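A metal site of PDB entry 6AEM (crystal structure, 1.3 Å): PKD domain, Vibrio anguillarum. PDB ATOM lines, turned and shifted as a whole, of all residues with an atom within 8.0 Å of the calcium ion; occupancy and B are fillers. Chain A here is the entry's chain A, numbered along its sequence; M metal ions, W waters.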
ATOM      1  N   GLU A   4       3.467  17.305  21.803  1.00  0.00           N
ATOM      2  CA  GLU A   4       3.360  17.872  23.133  1.00  0.00           C
ATOM      3  C   GLU A   4       1.937  17.717  23.607  1.00  0.00           C
ATOM      4  O   GLU A   4       1.409  18.556  24.333  1.00  0.00           O
ATOM      5  CB  GLU A   4       3.735  19.332  23.093  1.00  0.00           C
ATOM      6  CG  GLU A   4       3.099  20.041  21.922  1.00  0.00           C
ATOM      7  CD  GLU A   4       3.156  21.532  22.093  1.00  0.00           C
ATOM      8  OE1 GLU A   4       4.114  22.011  22.743  1.00  0.00           O
ATOM      9  OE2 GLU A   4       2.230  22.233  21.619  1.00  0.00           O
ATOM     10  N   ASN A   5       1.306  16.622  23.199  1.00  0.00           N
ATOM     11  CA  ASN A   5       0.023  16.263  23.785  1.00  0.00           C
ATOM     12  C   ASN A   5       0.110  16.208  25.309  1.00  0.00           C
ATOM     13  O   ASN A   5       1.071  15.679  25.879  1.00  0.00           O
ATOM     14  CB  ASN A   5      -0.396  14.891  23.285  1.00  0.00           C
ATOM     15  CG  ASN A   5      -1.706  14.450  23.876  1.00  0.00           C
ATOM     16  OD1 ASN A   5      -2.648  15.250  24.015  1.00  0.00           O
ATOM     17  ND2 ASN A   5      -1.768  13.188  24.287  1.00  0.00           N
ATOM     18  N   GLN A   6      -0.910  16.758  25.968  1.00  0.00           N
ATOM     19  CA  GLN A   6      -1.081  16.569  27.403  1.00  0.00           C
ATOM     20  C   GLN A   6      -1.914  15.316  27.654  1.00  0.00           C
ATOM     21  O   GLN A   6      -2.979  15.148  27.036  1.00  0.00           O
ATOM     22  CB  GLN A   6      -1.746  17.801  28.024  1.00  0.00           C
ATOM     23  CG  GLN A   6      -0.968  19.097  27.820  1.00  0.00           C
ATOM     24  CD  GLN A   6      -1.688  20.314  28.416  1.00  0.00           C
ATOM     25  OE1 GLN A   6      -2.146  20.294  29.575  1.00  0.00           O
ATOM     26  NE2 GLN A   6      -1.831  21.359  27.611  1.00  0.00           N
ATOM     27  N   ALA A   7      -1.431  14.401  28.507  1.00  0.00           N
ATOM     28  CA  ALA A   7      -2.210  13.232  28.871  1.00  0.00           C
ATOM     29  C   ALA A   7      -3.471  13.686  29.605  1.00  0.00           C
ATOM     30  O   ALA A   7      -3.466  14.716  30.294  1.00  0.00           O
ATOM     31  CB  ALA A   7      -1.401  12.297  29.755  1.00  0.00           C
ATOM     32  N   PRO A   8      -4.572  12.971  29.451  1.00  0.00           N
ATOM     33  CA  PRO A   8      -5.831  13.400  30.071  1.00  0.00           C
ATOM     34  C   PRO A   8      -5.755  13.332  31.581  1.00  0.00           C
ATOM     35  O   PRO A   8      -4.931  12.646  32.189  1.00  0.00           O
ATOM     36  CB  PRO A   8      -6.842  12.390  29.483  1.00  0.00           C
ATOM     37  CG  PRO A   8      -6.018  11.154  29.242  1.00  0.00           C
ATOM     38  CD  PRO A   8      -4.683  11.679  28.766  1.00  0.00           C
ATOM     39  N   VAL A   9      -6.686  14.047  32.192  1.00  0.00           N
ATOM     40  CA  VAL A   9      -6.844  14.111  33.649  1.00  0.00           C
ATOM     41  C   VAL A   9      -8.002  13.204  34.051  1.00  0.00           C
ATOM     42  O   VAL A   9      -9.121  13.396  33.619  1.00  0.00           O
ATOM     43  CB  VAL A   9      -7.133  15.546  34.114  1.00  0.00           C
ATOM     44  CG1 VAL A   9      -7.340  15.583  35.615  1.00  0.00           C
ATOM     45  CG2 VAL A   9      -6.028  16.502  33.695  1.00  0.00           C
ATOM     46  N   HIS A  28     -11.188  15.050  32.224  1.00  0.00           N
ATOM     47  CA  HIS A  28     -11.186  15.948  31.066  1.00  0.00           C
ATOM     48  C   HIS A  28      -9.809  15.918  30.454  1.00  0.00           C
ATOM     49  O   HIS A  28      -8.845  15.482  31.070  1.00  0.00           O
ATOM     50  CB  HIS A  28     -11.574  17.387  31.487  1.00  0.00           C
ATOM     51  CG  HIS A  28     -10.646  17.996  32.476  1.00  0.00           C
ATOM     52  ND1 HIS A  28     -10.625  17.640  33.809  1.00  0.00           N
ATOM     53  CD2 HIS A  28      -9.657  18.914  32.325  1.00  0.00           C
ATOM     54  CE1 HIS A  28      -9.683  18.315  34.424  1.00  0.00           C
ATOM     55  NE2 HIS A  28      -9.077  19.094  33.545  1.00  0.00           N
ATOM     56  N   ASP A  29      -9.730  16.425  29.227  1.00  0.00           N
ATOM     57  CA  ASP A  29      -8.457  16.579  28.515  1.00  0.00           C
ATOM     58  C   ASP A  29      -8.251  18.074  28.259  1.00  0.00           C
ATOM     59  O   ASP A  29      -9.087  18.717  27.614  1.00  0.00           O
ATOM     60  CB  ASP A  29      -8.484  15.773  27.212  1.00  0.00           C
ATOM     61  CG  ASP A  29      -7.116  15.618  26.567  1.00  0.00           C
ATOM     62  OD1 ASP A  29      -6.124  15.528  27.301  1.00  0.00           O
ATOM     63  OD2 ASP A  29      -7.046  15.537  25.327  1.00  0.00           O
ATOM     64  N   GLU A  30      -7.120  18.614  28.724  1.00  0.00           N
ATOM     65  CA  GLU A  30      -6.876  20.059  28.648  1.00  0.00           C
ATOM     66  C   GLU A  30      -6.732  20.542  27.226  1.00  0.00           C
ATOM     67  O   GLU A  30      -7.018  21.725  26.952  1.00  0.00           O
ATOM     68  CB  GLU A  30      -5.570  20.449  29.367  1.00  0.00           C
ATOM     69  CG  GLU A  30      -5.352  20.019  30.820  1.00  0.00           C
ATOM     70  CD  GLU A  30      -6.360  20.651  31.787  1.00  0.00           C
ATOM     71  OE1 GLU A  30      -7.369  21.161  31.303  1.00  0.00           O
ATOM     72  OE2 GLU A  30      -6.099  20.663  33.019  1.00  0.00           O
ATOM     73  N   ASP A  31      -6.244  19.680  26.323  1.00  0.00           N
ATOM     74  CA  ASP A  31      -5.894  20.054  24.963  1.00  0.00           C
ATOM     75  C   ASP A  31      -6.617  19.195  23.925  1.00  0.00           C
ATOM     76  O   ASP A  31      -6.141  19.083  22.795  1.00  0.00           O
ATOM     77  CB  ASP A  31      -4.377  19.984  24.731  1.00  0.00           C
ATOM     78  CG  ASP A  31      -3.799  18.591  24.882  1.00  0.00           C
ATOM     79  OD1 ASP A  31      -4.503  17.688  25.379  1.00  0.00           O
ATOM     80  OD2 ASP A  31      -2.613  18.428  24.539  1.00  0.00           O
ATOM     81  N   GLY A  32      -7.621  18.438  24.317  1.00  0.00           N
ATOM     82  CA  GLY A  32      -8.327  17.589  23.377  1.00  0.00           C
ATOM     83  C   GLY A  32      -9.645  17.117  23.925  1.00  0.00           C
ATOM     84  O   GLY A  32     -10.346  17.865  24.623  1.00  0.00           O
ATOM     85  N   GLU A  33      -9.949  15.848  23.705  1.00  0.00           N
ATOM     86  CA  GLU A  33     -11.211  15.273  24.161  1.00  0.00           C
ATOM     87  C   GLU A  33     -10.966  13.875  24.713  1.00  0.00           C
ATOM     88  O   GLU A  33     -10.000  13.200  24.322  1.00  0.00           O
ATOM     89  CB  GLU A  33     -12.225  15.148  23.003  1.00  0.00           C
ATOM     90  CG  GLU A  33     -12.561  16.485  22.312  1.00  0.00           C
ATOM     91  CD  GLU A  33     -13.342  17.481  23.179  1.00  0.00           C
ATOM     92  OE1 GLU A  33     -13.885  17.088  24.217  1.00  0.00           O
ATOM     93  OE2 GLU A  33     -13.450  18.671  22.789  1.00  0.00           O
ATOM     94  N   LEU A  34     -11.830  13.445  25.612  1.00  0.00           N
ATOM     95  CA  LEU A  34     -11.854  12.066  26.088  1.00  0.00           C
ATOM     96  C   LEU A  34     -12.675  11.204  25.141  1.00  0.00           C
ATOM     97  O   LEU A  34     -13.747  11.609  24.707  1.00  0.00           O
ATOM     98  CB  LEU A  34     -12.471  11.976  27.481  1.00  0.00           C
ATOM     99  CG  LEU A  34     -11.695  12.735  28.548  1.00  0.00           C
ATOM    100  CD1 LEU A  34     -12.326  12.495  29.937  1.00  0.00           C
ATOM    101  CD2 LEU A  34     -10.209  12.412  28.565  1.00  0.00           C
ATOM    102  N   THR A  69      -9.025   7.802  28.366  1.00  0.00           N
ATOM    103  CA  THR A  69      -8.197   7.861  27.159  1.00  0.00           C
ATOM    104  C   THR A  69      -8.555   9.103  26.352  1.00  0.00           C
ATOM    105  O   THR A  69      -9.735   9.390  26.168  1.00  0.00           O
ATOM    106  CB  THR A  69      -8.436   6.594  26.276  1.00  0.00           C
ATOM    107  OG1 THR A  69      -8.217   5.416  27.065  1.00  0.00           O
ATOM    108  CG2 THR A  69      -7.524   6.542  25.067  1.00  0.00           C
ATOM    109  N   ASP A  70      -7.555   9.804  25.817  1.00  0.00           N
ATOM    110  CA  ASP A  70      -7.802  10.996  25.009  1.00  0.00           C
ATOM    111  C   ASP A  70      -7.807  10.656  23.502  1.00  0.00           C
ATOM    112  O   ASP A  70      -7.675   9.506  23.084  1.00  0.00           O
ATOM    113  CB  ASP A  70      -6.898  12.184  25.382  1.00  0.00           C
ATOM    114  CG  ASP A  70      -5.461  12.063  24.849  1.00  0.00           C
ATOM    115  OD1 ASP A  70      -5.136  11.148  24.046  1.00  0.00           O
ATOM    116  OD2 ASP A  70      -4.650  12.928  25.287  1.00  0.00           O
ATOM    117  N   ASP A  71      -8.025  11.700  22.687  1.00  0.00           N
ATOM    118  CA  ASP A  71      -8.162  11.611  21.239  1.00  0.00           C
ATOM    119  C   ASP A  71      -6.888  11.170  20.533  1.00  0.00           C
ATOM    120  O   ASP A  71      -6.949  10.817  19.355  1.00  0.00           O
ATOM    121  CB  ASP A  71      -8.641  12.951  20.656  1.00  0.00           C
ATOM    122  CG  ASP A  71      -7.729  14.110  21.042  1.00  0.00           C
ATOM    123  OD1 ASP A  71      -7.690  14.487  22.222  1.00  0.00           O
ATOM    124  OD2 ASP A  71      -7.083  14.652  20.138  1.00  0.00           O
ATOM    125  N   LYS A  72      -5.752  11.187  21.248  1.00  0.00           N
ATOM    126  CA  LYS A  72      -4.484  10.693  20.711  1.00  0.00           C
ATOM    127  C   LYS A  72      -4.088   9.330  21.256  1.00  0.00           C
ATOM    128  O   LYS A  72      -3.038   8.773  20.878  1.00  0.00           O
ATOM    129  CB  LYS A  72      -3.373  11.717  20.996  1.00  0.00           C
ATOM    130  CG  LYS A  72      -3.672  13.107  20.489  1.00  0.00           C
ATOM    131  CD  LYS A  72      -3.707  13.165  18.998  1.00  0.00           C
ATOM    132  CE  LYS A  72      -3.882  14.612  18.507  1.00  0.00           C
ATOM    133  NZ  LYS A  72      -4.303  14.635  17.093  1.00  0.00           N
ATOM    134  N   GLY A  73      -4.900   8.750  22.139  1.00  0.00           N
ATOM    135  CA  GLY A  73      -4.628   7.462  22.736  1.00  0.00           C
ATOM    136  C   GLY A  73      -3.856   7.507  24.040  1.00  0.00           C
ATOM    137  O   GLY A  73      -3.575   6.454  24.595  1.00  0.00           O
ATOM    138  N   ALA A  74      -3.579   8.689  24.563  1.00  0.00           N
ATOM    139  CA  ALA A  74      -2.903   8.779  25.852  1.00  0.00           C
ATOM    140  C   ALA A  74      -3.899   8.477  26.962  1.00  0.00           C
ATOM    141  O   ALA A  74      -5.098   8.713  26.841  1.00  0.00           O
ATOM    142  CB  ALA A  74      -2.310  10.165  26.074  1.00  0.00           C
ATOM    143  N   THR A  75      -3.384   7.944  28.083  1.00  0.00           N
ATOM    144  CA  THR A  75      -4.223   7.511  29.192  1.00  0.00           C
ATOM    145  C   THR A  75      -3.732   8.056  30.530  1.00  0.00           C
ATOM    146  O   THR A  75      -2.623   8.545  30.661  1.00  0.00           O
ATOM    147  CB  THR A  75      -4.298   5.979  29.305  1.00  0.00           C
ATOM    148  OG1 THR A  75      -2.991   5.446  29.536  1.00  0.00           O
ATOM    149  CG2 THR A  75      -4.804   5.366  28.001  1.00  0.00           C
HETATM  150 CA    CA M   1      -4.607  15.340  25.350  1.00  0.00          CA
HETATM  151  O   HOH W   1      -5.265  15.350  23.049  1.00  0.00           O
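The side-chain carboxylate of Asp 29 lies close to the backbone NH of Gly 32 (3.1 Å).
OD2 of Asp 29 sits close to N of Glu 33 (3.3 Å).
OD1 of Asp 70 is in hydrogen-bond range of N of Gly 73, 3.1 Å away.
The side-chain carboxylate (OD1) of Asp 70 is in hydrogen-bond range of the backbone NH (N) of Ala 74 (3.0 Å).
The backbone NH (N) of Lys 72 sits at hydrogen-bond distance from the side-chain carboxylate (OD1) of Asp 70, at 2.9 Å.
The calcium ion is bound by the side-chain carboxylate (OD1) of Asp 31 (2.4 Å), the backbone carbonyl oxygen (O) of Gln 6 (2.4 Å), the side-chain amide oxygen (OD1) of Asn 5 (2.4 Å), water W1 (2.4 Å), the side-chain carboxylate (OD2) of Asp 70 (2.4 Å), the side-chain carboxylate (OD2) of Asp 29 (2.4 Å) and the side-chain carboxylate (OD1) of Asp 29 (2.5 Å).
The calcium ion has seven donor atoms within binding distance.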
